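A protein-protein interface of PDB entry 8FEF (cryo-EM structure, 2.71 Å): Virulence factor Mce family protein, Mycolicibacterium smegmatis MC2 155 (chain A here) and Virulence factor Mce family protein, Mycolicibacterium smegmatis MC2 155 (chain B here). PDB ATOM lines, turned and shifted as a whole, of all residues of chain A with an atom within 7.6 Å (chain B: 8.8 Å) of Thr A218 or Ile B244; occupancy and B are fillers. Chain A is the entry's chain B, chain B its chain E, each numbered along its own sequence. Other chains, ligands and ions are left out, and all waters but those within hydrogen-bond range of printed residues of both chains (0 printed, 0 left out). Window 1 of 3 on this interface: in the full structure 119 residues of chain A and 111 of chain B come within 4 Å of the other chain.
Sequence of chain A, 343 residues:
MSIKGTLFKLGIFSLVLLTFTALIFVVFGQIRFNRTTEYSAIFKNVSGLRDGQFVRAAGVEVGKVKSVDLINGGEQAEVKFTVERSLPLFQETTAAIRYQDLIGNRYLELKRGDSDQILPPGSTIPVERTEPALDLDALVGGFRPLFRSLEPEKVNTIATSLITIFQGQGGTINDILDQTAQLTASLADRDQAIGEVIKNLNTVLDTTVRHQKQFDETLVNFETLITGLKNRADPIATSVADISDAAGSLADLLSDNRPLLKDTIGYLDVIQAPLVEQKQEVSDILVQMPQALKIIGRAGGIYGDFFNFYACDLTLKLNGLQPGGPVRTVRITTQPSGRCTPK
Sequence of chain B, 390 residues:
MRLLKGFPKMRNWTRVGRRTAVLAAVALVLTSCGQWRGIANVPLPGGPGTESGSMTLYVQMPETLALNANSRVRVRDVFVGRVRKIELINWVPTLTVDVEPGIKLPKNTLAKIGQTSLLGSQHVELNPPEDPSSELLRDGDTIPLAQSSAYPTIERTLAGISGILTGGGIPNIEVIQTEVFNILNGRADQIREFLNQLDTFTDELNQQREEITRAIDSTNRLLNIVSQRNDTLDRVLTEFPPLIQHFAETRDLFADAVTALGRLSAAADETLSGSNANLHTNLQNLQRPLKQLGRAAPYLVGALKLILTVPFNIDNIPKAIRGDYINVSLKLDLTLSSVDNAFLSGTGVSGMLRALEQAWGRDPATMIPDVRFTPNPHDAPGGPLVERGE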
ATOM      1  N   HIS A 211       1.230   6.670   6.149  1.00  0.00           N
ATOM      2  CA  HIS A 211       0.343   5.948   7.053  1.00  0.00           C
ATOM      3  C   HIS A 211       0.013   4.549   6.535  1.00  0.00           C
ATOM      4  O   HIS A 211      -1.097   4.056   6.743  1.00  0.00           O
ATOM      5  CB  HIS A 211      -0.942   6.742   7.276  1.00  0.00           C
ATOM      6  CG  HIS A 211      -0.708   8.186   7.590  1.00  0.00           C
ATOM      7  ND1 HIS A 211      -0.632   9.153   6.611  1.00  0.00           N
ATOM      8  CD2 HIS A 211      -0.523   8.827   8.767  1.00  0.00           C
ATOM      9  CE1 HIS A 211      -0.417  10.329   7.173  1.00  0.00           C
ATOM     10  NE2 HIS A 211      -0.345  10.158   8.481  1.00  0.00           N
ATOM     11  N   GLN A 212       0.968   3.909   5.849  1.00  0.00           N
ATOM     12  CA  GLN A 212       0.710   2.616   5.218  1.00  0.00           C
ATOM     13  C   GLN A 212       0.286   1.558   6.230  1.00  0.00           C
ATOM     14  O   GLN A 212      -0.575   0.722   5.938  1.00  0.00           O
ATOM     15  CB  GLN A 212       1.948   2.153   4.451  1.00  0.00           C
ATOM     16  CG  GLN A 212       1.825   0.770   3.845  1.00  0.00           C
ATOM     17  CD  GLN A 212       3.078   0.338   3.120  1.00  0.00           C
ATOM     18  OE1 GLN A 212       3.824   1.166   2.598  1.00  0.00           O
ATOM     19  NE2 GLN A 212       3.322  -0.967   3.087  1.00  0.00           N
ATOM     20  N   LYS A 213       0.886   1.570   7.422  1.00  0.00           N
ATOM     21  CA  LYS A 213       0.505   0.616   8.459  1.00  0.00           C
ATOM     22  C   LYS A 213      -0.953   0.804   8.870  1.00  0.00           C
ATOM     23  O   LYS A 213      -1.726  -0.161   8.935  1.00  0.00           O
ATOM     24  CB  LYS A 213       1.432   0.774   9.665  1.00  0.00           C
ATOM     25  CG  LYS A 213       1.279  -0.289  10.738  1.00  0.00           C
ATOM     26  CD  LYS A 213       1.821  -1.626  10.268  1.00  0.00           C
ATOM     27  CE  LYS A 213       2.095  -2.551  11.441  1.00  0.00           C
ATOM     28  NZ  LYS A 213       0.894  -2.729  12.301  1.00  0.00           N
ATOM     29  N   GLN A 214      -1.348   2.052   9.130  1.00  0.00           N
ATOM     30  CA  GLN A 214      -2.727   2.336   9.512  1.00  0.00           C
ATOM     31  C   GLN A 214      -3.687   2.099   8.353  1.00  0.00           C
ATOM     32  O   GLN A 214      -4.794   1.589   8.555  1.00  0.00           O
ATOM     33  CB  GLN A 214      -2.841   3.773  10.018  1.00  0.00           C
ATOM     34  CG  GLN A 214      -1.665   4.227  10.869  1.00  0.00           C
ATOM     35  CD  GLN A 214      -1.397   3.305  12.043  1.00  0.00           C
ATOM     36  OE1 GLN A 214      -2.321   2.852  12.718  1.00  0.00           O
ATOM     37  NE2 GLN A 214      -0.124   3.018  12.288  1.00  0.00           N
ATOM     38  N   PHE A 215      -3.283   2.469   7.136  1.00  0.00           N
ATOM     39  CA  PHE A 215      -4.116   2.222   5.963  1.00  0.00           C
ATOM     40  C   PHE A 215      -4.324   0.732   5.725  1.00  0.00           C
ATOM     41  O   PHE A 215      -5.381   0.323   5.234  1.00  0.00           O
ATOM     42  CB  PHE A 215      -3.486   2.885   4.737  1.00  0.00           C
ATOM     43  CG  PHE A 215      -4.196   2.589   3.449  1.00  0.00           C
ATOM     44  CD1 PHE A 215      -5.458   3.100   3.204  1.00  0.00           C
ATOM     45  CD2 PHE A 215      -3.591   1.817   2.472  1.00  0.00           C
ATOM     46  CE1 PHE A 215      -6.110   2.834   2.016  1.00  0.00           C
ATOM     47  CE2 PHE A 215      -4.238   1.548   1.283  1.00  0.00           C
ATOM     48  CZ  PHE A 215      -5.498   2.058   1.055  1.00  0.00           C
ATOM     49  N   ASP A 216      -3.329  -0.091   6.055  1.00  0.00           N
ATOM     50  CA  ASP A 216      -3.481  -1.535   5.922  1.00  0.00           C
ATOM     51  C   ASP A 216      -4.372  -2.101   7.019  1.00  0.00           C
ATOM     52  O   ASP A 216      -5.222  -2.957   6.753  1.00  0.00           O
ATOM     53  CB  ASP A 216      -2.107  -2.205   5.944  1.00  0.00           C
ATOM     54  CG  ASP A 216      -2.192  -3.715   5.862  1.00  0.00           C
ATOM     55  OD1 ASP A 216      -2.375  -4.241   4.746  1.00  0.00           O
ATOM     56  OD2 ASP A 216      -2.075  -4.378   6.915  1.00  0.00           O
ATOM     57  N   GLU A 217      -4.188  -1.640   8.260  1.00  0.00           N
ATOM     58  CA  GLU A 217      -4.977  -2.170   9.370  1.00  0.00           C
ATOM     59  C   GLU A 217      -6.444  -1.760   9.290  1.00  0.00           C
ATOM     60  O   GLU A 217      -7.321  -2.530   9.710  1.00  0.00           O
ATOM     61  CB  GLU A 217      -4.386  -1.721  10.704  1.00  0.00           C
ATOM     62  CG  GLU A 217      -3.019  -2.302  11.015  1.00  0.00           C
ATOM     63  CD  GLU A 217      -2.517  -1.894  12.387  1.00  0.00           C
ATOM     64  OE1 GLU A 217      -3.306  -1.314  13.162  1.00  0.00           O
ATOM     65  OE2 GLU A 217      -1.336  -2.154  12.692  1.00  0.00           O
ATOM     66  N   THR A 218      -6.732  -0.561   8.775  1.00  0.00           N
ATOM     67  CA  THR A 218      -8.107  -0.077   8.791  1.00  0.00           C
ATOM     68  C   THR A 218      -9.004  -0.876   7.856  1.00  0.00           C
ATOM     69  O   THR A 218     -10.195  -1.016   8.133  1.00  0.00           O
ATOM     70  CB  THR A 218      -8.165   1.416   8.449  1.00  0.00           C
ATOM     71  OG1 THR A 218      -9.517   1.875   8.557  1.00  0.00           O
ATOM     72  CG2 THR A 218      -7.667   1.686   7.042  1.00  0.00           C
ATOM     73  N   LEU A 219      -8.461  -1.422   6.763  1.00  0.00           N
ATOM     74  CA  LEU A 219      -9.271  -2.258   5.880  1.00  0.00           C
ATOM     75  C   LEU A 219      -9.757  -3.507   6.608  1.00  0.00           C
ATOM     76  O   LEU A 219     -10.947  -3.843   6.565  1.00  0.00           O
ATOM     77  CB  LEU A 219      -8.472  -2.641   4.634  1.00  0.00           C
ATOM     78  CG  LEU A 219      -7.998  -1.494   3.744  1.00  0.00           C
ATOM     79  CD1 LEU A 219      -7.257  -2.035   2.534  1.00  0.00           C
ATOM     80  CD2 LEU A 219      -9.172  -0.633   3.318  1.00  0.00           C
ATOM     81  N   VAL A 220      -8.847  -4.197   7.297  1.00  0.00           N
ATOM     82  CA  VAL A 220      -9.215  -5.403   8.031  1.00  0.00           C
ATOM     83  C   VAL A 220     -10.166  -5.069   9.172  1.00  0.00           C
ATOM     84  O   VAL A 220     -11.141  -5.792   9.416  1.00  0.00           O
ATOM     85  CB  VAL A 220      -7.953  -6.122   8.540  1.00  0.00           C
ATOM     86  CG1 VAL A 220      -8.315  -7.472   9.138  1.00  0.00           C
ATOM     87  CG2 VAL A 220      -6.946  -6.278   7.417  1.00  0.00           C
ATOM     88  N   ASN A 221      -9.898  -3.977   9.898  1.00  0.00           N
ATOM     89  CA  ASN A 221     -10.771  -3.607  11.009  1.00  0.00           C
ATOM     90  C   ASN A 221     -12.168  -3.242  10.522  1.00  0.00           C
ATOM     91  O   ASN A 221     -13.171  -3.631  11.135  1.00  0.00           O
ATOM     92  CB  ASN A 221     -10.157  -2.454  11.802  1.00  0.00           C
ATOM     93  CG  ASN A 221      -8.897  -2.859  12.536  1.00  0.00           C
ATOM     94  OD1 ASN A 221      -7.882  -2.166  12.482  1.00  0.00           O
ATOM     95  ND2 ASN A 221      -8.953  -3.991  13.229  1.00  0.00           N
ATOM     96  N   PHE A 222     -12.255  -2.496   9.417  1.00  0.00           N
ATOM     97  CA  PHE A 222     -13.548  -2.135   8.854  1.00  0.00           C
ATOM     98  C   PHE A 222     -14.293  -3.367   8.366  1.00  0.00           C
ATOM     99  O   PHE A 222     -15.510  -3.478   8.554  1.00  0.00           O
ATOM    100  CB  PHE A 222     -13.354  -1.138   7.714  1.00  0.00           C
ATOM    101  CG  PHE A 222     -14.453  -0.125   7.600  1.00  0.00           C
ATOM    102  CD1 PHE A 222     -15.604  -0.241   8.358  1.00  0.00           C
ATOM    103  CD2 PHE A 222     -14.334   0.944   6.730  1.00  0.00           C
ATOM    104  CE1 PHE A 222     -16.613   0.690   8.255  1.00  0.00           C
ATOM    105  CE2 PHE A 222     -15.341   1.877   6.621  1.00  0.00           C
ATOM    106  CZ  PHE A 222     -16.483   1.749   7.383  1.00  0.00           C
ATOM    107  N   GLU A 223     -13.581  -4.302   7.729  1.00  0.00           N
ATOM    108  CA  GLU A 223     -14.214  -5.538   7.286  1.00  0.00           C
ATOM    109  C   GLU A 223     -14.767  -6.324   8.466  1.00  0.00           C
ATOM    110  O   GLU A 223     -15.897  -6.822   8.410  1.00  0.00           O
ATOM    111  CB  GLU A 223     -13.217  -6.381   6.489  1.00  0.00           C
ATOM    112  CG  GLU A 223     -13.776  -7.689   5.939  1.00  0.00           C
ATOM    113  CD  GLU A 223     -13.609  -8.859   6.891  1.00  0.00           C
ATOM    114  OE1 GLU A 223     -12.709  -8.802   7.754  1.00  0.00           O
ATOM    115  OE2 GLU A 223     -14.379  -9.836   6.779  1.00  0.00           O
ATOM    116  N   THR A 224     -13.991  -6.436   9.545  1.00  0.00           N
ATOM    117  CA  THR A 224     -14.458  -7.162  10.725  1.00  0.00           C
ATOM    118  C   THR A 224     -15.686  -6.494  11.331  1.00  0.00           C
ATOM    119  O   THR A 224     -16.673  -7.165  11.661  1.00  0.00           O
ATOM    120  CB  THR A 224     -13.337  -7.257  11.759  1.00  0.00           C
ATOM    121  OG1 THR A 224     -12.169  -7.820  11.150  1.00  0.00           O
ATOM    122  CG2 THR A 224     -13.764  -8.132  12.925  1.00  0.00           C
ATOM    123  N   LEU A 225     -15.648  -5.165  11.470  1.00  0.00           N
ATOM    124  CA  LEU A 225     -16.773  -4.439  12.053  1.00  0.00           C
ATOM    125  C   LEU A 225     -18.029  -4.589  11.203  1.00  0.00           C
ATOM    126  O   LEU A 225     -19.120  -4.854  11.723  1.00  0.00           O
ATOM    127  CB  LEU A 225     -16.405  -2.964  12.214  1.00  0.00           C
ATOM    128  CG  LEU A 225     -17.544  -1.988  12.510  1.00  0.00           C
ATOM    129  CD1 LEU A 225     -18.160  -2.271  13.867  1.00  0.00           C
ATOM    130  CD2 LEU A 225     -17.047  -0.559  12.429  1.00  0.00           C
ATOM    131  N   VAL B 236      -7.478  12.432   8.137  1.00  0.00           N
ATOM    132  CA  VAL B 236      -8.274  11.208   8.142  1.00  0.00           C
ATOM    133  C   VAL B 236      -7.385  10.009   8.435  1.00  0.00           C
ATOM    134  O   VAL B 236      -7.660   9.216   9.343  1.00  0.00           O
ATOM    135  CB  VAL B 236      -9.017  11.039   6.804  1.00  0.00           C
ATOM    136  CG1 VAL B 236      -9.636   9.654   6.715  1.00  0.00           C
ATOM    137  CG2 VAL B 236     -10.087  12.100   6.648  1.00  0.00           C
ATOM    138  N   LEU B 237      -6.276   9.885   7.696  1.00  0.00           N
ATOM    139  CA  LEU B 237      -5.391   8.739   7.864  1.00  0.00           C
ATOM    140  C   LEU B 237      -4.709   8.708   9.226  1.00  0.00           C
ATOM    141  O   LEU B 237      -4.145   7.673   9.591  1.00  0.00           O
ATOM    142  CB  LEU B 237      -4.339   8.717   6.758  1.00  0.00           C
ATOM    143  CG  LEU B 237      -4.801   8.117   5.430  1.00  0.00           C
ATOM    144  CD1 LEU B 237      -3.667   8.109   4.425  1.00  0.00           C
ATOM    145  CD2 LEU B 237      -5.333   6.713   5.650  1.00  0.00           C
ATOM    146  N   GLU B 239      -6.486  10.022  12.219  1.00  0.00           N
ATOM    147  CA  GLU B 239      -7.470   9.969  13.293  1.00  0.00           C
ATOM    148  C   GLU B 239      -8.555   8.915  13.115  1.00  0.00           C
ATOM    149  O   GLU B 239      -9.171   8.522  14.113  1.00  0.00           O
ATOM    150  CB  GLU B 239      -8.121  11.345  13.467  1.00  0.00           C
ATOM    151  CG  GLU B 239      -7.114  12.440  13.787  1.00  0.00           C
ATOM    152  CD  GLU B 239      -7.767  13.718  14.263  1.00  0.00           C
ATOM    153  OE1 GLU B 239      -8.995  13.710  14.474  1.00  0.00           O
ATOM    154  OE2 GLU B 239      -7.050  14.727  14.429  1.00  0.00           O
ATOM    155  N   PHE B 240      -8.825   8.451  11.896  1.00  0.00           N
ATOM    156  CA  PHE B 240      -9.878   7.457  11.699  1.00  0.00           C
ATOM    157  C   PHE B 240      -9.476   6.008  11.995  1.00  0.00           C
ATOM    158  O   PHE B 240     -10.305   5.280  12.559  1.00  0.00           O
ATOM    159  CB  PHE B 240     -10.441   7.560  10.281  1.00  0.00           C
ATOM    160  CG  PHE B 240     -11.717   8.340  10.202  1.00  0.00           C
ATOM    161  CD1 PHE B 240     -12.911   7.770  10.604  1.00  0.00           C
ATOM    162  CD2 PHE B 240     -11.723   9.643   9.739  1.00  0.00           C
ATOM    163  CE1 PHE B 240     -14.089   8.481  10.540  1.00  0.00           C
ATOM    164  CE2 PHE B 240     -12.899  10.361   9.672  1.00  0.00           C
ATOM    165  CZ  PHE B 240     -14.083   9.777  10.074  1.00  0.00           C
ATOM    166  N   PRO B 241      -8.290   5.523  11.605  1.00  0.00           N
ATOM    167  CA  PRO B 241      -7.955   4.104  11.849  1.00  0.00           C
ATOM    168  C   PRO B 241      -8.067   3.700  13.314  1.00  0.00           C
ATOM    169  O   PRO B 241      -8.541   2.588  13.588  1.00  0.00           O
ATOM    170  CB  PRO B 241      -6.512   3.988  11.336  1.00  0.00           C
ATOM    171  CG  PRO B 241      -6.450   4.966  10.254  1.00  0.00           C
ATOM    172  CD  PRO B 241      -7.295   6.130  10.693  1.00  0.00           C
ATOM    173  N   PRO B 242      -7.637   4.527  14.291  1.00  0.00           N
ATOM    174  CA  PRO B 242      -7.882   4.126  15.691  1.00  0.00           C
ATOM    175  C   PRO B 242      -9.356   3.981  16.028  1.00  0.00           C
ATOM    176  O   PRO B 242      -9.739   3.042  16.738  1.00  0.00           O
ATOM    177  CB  PRO B 242      -7.224   5.250  16.500  1.00  0.00           C
ATOM    178  CG  PRO B 242      -6.191   5.784  15.615  1.00  0.00           C
ATOM    179  CD  PRO B 242      -6.786   5.735  14.250  1.00  0.00           C
ATOM    180  N   LEU B 243     -10.196   4.891  15.527  1.00  0.00           N
ATOM    181  CA  LEU B 243     -11.631   4.804  15.778  1.00  0.00           C
ATOM    182  C   LEU B 243     -12.220   3.539  15.170  1.00  0.00           C
ATOM    183  O   LEU B 243     -13.033   2.857  15.805  1.00  0.00           O
ATOM    184  CB  LEU B 243     -12.330   6.042  15.217  1.00  0.00           C
ATOM    185  CG  LEU B 243     -13.840   6.133  15.426  1.00  0.00           C
ATOM    186  CD1 LEU B 243     -14.156   6.407  16.885  1.00  0.00           C
ATOM    187  CD2 LEU B 243     -14.441   7.200  14.530  1.00  0.00           C
ATOM    188  N   ILE B 244     -11.818   3.211  13.940  1.00  0.00           N
ATOM    189  CA  ILE B 244     -12.341   2.022  13.275  1.00  0.00           C
ATOM    190  C   ILE B 244     -11.874   0.761  13.991  1.00  0.00           C
ATOM    191  O   ILE B 244     -12.643  -0.195  14.155  1.00  0.00           O
ATOM    192  CB  ILE B 244     -11.940   2.026  11.789  1.00  0.00           C
ATOM    193  CG1 ILE B 244     -12.566   3.228  11.082  1.00  0.00           C
ATOM    194  CG2 ILE B 244     -12.367   0.739  11.112  1.00  0.00           C
ATOM    195  CD1 ILE B 244     -12.283   3.286   9.601  1.00  0.00           C
ATOM    196  N   GLN B 245     -10.614   0.739  14.436  1.00  0.00           N
ATOM    197  CA  GLN B 245     -10.115  -0.402  15.195  1.00  0.00           C
ATOM    198  C   GLN B 245     -10.890  -0.579  16.493  1.00  0.00           C
ATOM    199  O   GLN B 245     -11.269  -1.703  16.849  1.00  0.00           O
ATOM    200  CB  GLN B 245      -8.624  -0.231  15.483  1.00  0.00           C
ATOM    201  CG  GLN B 245      -8.056  -1.286  16.418  1.00  0.00           C
ATOM    202  CD  GLN B 245      -6.575  -1.104  16.673  1.00  0.00           C
ATOM    203  OE1 GLN B 245      -5.937  -0.220  16.102  1.00  0.00           O
ATOM    204  NE2 GLN B 245      -6.018  -1.944  17.536  1.00  0.00           N
ATOM    205  N   HIS B 246     -11.142   0.518  17.212  1.00  0.00           N
ATOM    206  CA  HIS B 246     -11.907   0.421  18.450  1.00  0.00           C
ATOM    207  C   HIS B 246     -13.323  -0.071  18.188  1.00  0.00           C
ATOM    208  O   HIS B 246     -13.833  -0.922  18.923  1.00  0.00           O
ATOM    209  CB  HIS B 246     -11.947   1.767  19.167  1.00  0.00           C
ATOM    210  CG  HIS B 246     -12.791   1.759  20.402  1.00  0.00           C
ATOM    211  ND1 HIS B 246     -12.534   0.930  21.473  1.00  0.00           N
ATOM    212  CD2 HIS B 246     -13.897   2.467  20.733  1.00  0.00           C
ATOM    213  CE1 HIS B 246     -13.439   1.133  22.412  1.00  0.00           C
ATOM    214  NE2 HIS B 246     -14.278   2.061  21.988  1.00  0.00           N
ATOM    215  N   PHE B 247     -13.969   0.447  17.139  1.00  0.00           N
ATOM    216  CA  PHE B 247     -15.325   0.014  16.815  1.00  0.00           C
ATOM    217  C   PHE B 247     -15.361  -1.468  16.468  1.00  0.00           C
ATOM    218  O   PHE B 247     -16.284  -2.184  16.870  1.00  0.00           O
ATOM    219  CB  PHE B 247     -15.887   0.849  15.664  1.00  0.00           C
ATOM    220  CG  PHE B 247     -16.371   2.207  16.079  1.00  0.00           C
ATOM    221  CD1 PHE B 247     -16.488   2.539  17.418  1.00  0.00           C
ATOM    222  CD2 PHE B 247     -16.725   3.148  15.128  1.00  0.00           C
ATOM    223  CE1 PHE B 247     -16.939   3.788  17.799  1.00  0.00           C
ATOM    224  CE2 PHE B 247     -17.176   4.397  15.504  1.00  0.00           C
ATOM    225  CZ  PHE B 247     -17.285   4.717  16.841  1.00  0.00           C
ATOM    226  N   ALA B 248     -14.365  -1.944  15.715  1.00  0.00           N
ATOM    227  CA  ALA B 248     -14.272  -3.369  15.425  1.00  0.00           C
ATOM    228  C   ALA B 248     -14.047  -4.183  16.690  1.00  0.00           C
ATOM    229  O   ALA B 248     -14.515  -5.323  16.786  1.00  0.00           O
ATOM    230  CB  ALA B 248     -13.151  -3.631  14.421  1.00  0.00           C
ATOM    231  N   GLU B 249     -13.324  -3.626  17.664  1.00  0.00           N
ATOM    232  CA  GLU B 249     -13.109  -4.339  18.920  1.00  0.00           C
ATOM    233  C   GLU B 249     -14.401  -4.484  19.718  1.00  0.00           C
ATOM    234  O   GLU B 249     -14.610  -5.507  20.383  1.00  0.00           O
ATOM    235  CB  GLU B 249     -12.043  -3.628  19.754  1.00  0.00           C
ATOM    236  CG  GLU B 249     -10.627  -3.768  19.217  1.00  0.00           C
ATOM    237  CD  GLU B 249     -10.058  -5.162  19.411  1.00  0.00           C
ATOM    238  OE1 GLU B 249     -10.558  -5.895  20.288  1.00  0.00           O
ATOM    239  OE2 GLU B 249      -9.108  -5.523  18.684  1.00  0.00           O
ATOM    240  N   THR B 250     -15.282  -3.481  19.671  1.00  0.00           N
ATOM    241  CA  THR B 250     -16.481  -3.465  20.503  1.00  0.00           C
ATOM    242  C   THR B 250     -17.765  -3.514  19.674  1.00  0.00           C
ATOM    243  O   THR B 250     -18.795  -2.971  20.079  1.00  0.00           O
ATOM    244  CB  THR B 250     -16.477  -2.244  21.426  1.00  0.00           C
ATOM    245  OG1 THR B 250     -17.638  -2.270  22.263  1.00  0.00           O
ATOM    246  CG2 THR B 250     -16.467  -0.948  20.629  1.00  0.00           C
ATOM    247  N   ARG B 251     -17.719  -4.181  18.517  1.00  0.00           N
ATOM    248  CA  ARG B 251     -18.914  -4.325  17.688  1.00  0.00           C
ATOM    249  C   ARG B 251     -20.004  -5.109  18.409  1.00  0.00           C
ATOM    250  O   ARG B 251     -21.191  -4.767  18.319  1.00  0.00           O
ATOM    251  CB  ARG B 251     -18.553  -5.008  16.370  1.00  0.00           C
ATOM    252  CG  ARG B 251     -17.629  -6.201  16.548  1.00  0.00           C
ATOM    253  CD  ARG B 251     -17.334  -6.906  15.242  1.00  0.00           C
ATOM    254  NE  ARG B 251     -16.199  -7.812  15.379  1.00  0.00           N
ATOM    255  CZ  ARG B 251     -16.267  -9.029  15.898  1.00  0.00           C
ATOM    256  NH1 ARG B 251     -17.410  -9.530  16.338  1.00  0.00           N
ATOM    257  NH2 ARG B 251     -15.161  -9.763  15.980  1.00  0.00           N
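The backbone carbonyl oxygen (O) of Glu A217 lies close to the side-chain amide oxygen (OD1) of Asn A221, at 2.9 Å. OG1 of Thr A224 lies within hydrogen-bond range of O of Val A220, 2.9 Å away. The backbone carbonyl oxygen (O) of Ala B248 lies close to the guanidinium group (NE) of Arg B251 (3.3 Å).
ND1 of His A211 touches CB of Leu B237, at 3.7 Å. CB of Gln A214 touches CG of Pro B241, at 3.8 Å. Ile B244 touches Thr A218 (CD1 to OG1, 3.3 Å). CG2 of Ile B244 touches CB of Asn A221, 3.9 Å away. Asn A221 touches Ala B248. Ile B244 touches Phe A222. CG2 of Thr A224 touches NE of Arg B251, at 3.5 Å. CD1 of Leu A225 touches O of Phe B247, 3.5 Å away. Leu A225 touches Ala B248 (CB to CA, 3.9 Å). CD1 of Leu A225 touches CB of Arg B251, 3.7 Å away.
Of the printed residues of chain B, His A211 touches Leu B237. Of chain B, only Ile B244 comes within 4 Å of Thr A218. Of the printed residues of chain A, Gln B245 touches Asn A221. Printed residues of chain A within 4 Å of Phe B247: Leu A225 (3.5 Å). Of the printed residues of chain A, Ala B248 touches Asn A221 and Leu A225. Thr B250 touches none of the printed residues of chain A. Printed residues of chain A within 4 Å of Arg B251: Thr A224 (3.5 Å) and Leu A225 (3.7 Å). The nearest printed residue of chain B that does not touch His A211 is Pro B241 (6.5 Å).
Hydrophobic or aromatic side chains of chain A within 4 Å of the printed part of chain B: His A211 and Leu A225. Hydrophobic or aromatic side chains of chain B that line the printed part of chain A: Leu B237, Pro B241, Ile B244, Phe B247 and Ala B248. Among the printed residues, 11 pairs touch across the chains. Among the printed residues, no Asp or Glu carboxylate lies within 4 Å of a Lys or Arg side-chain nitrogen of the other chain.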
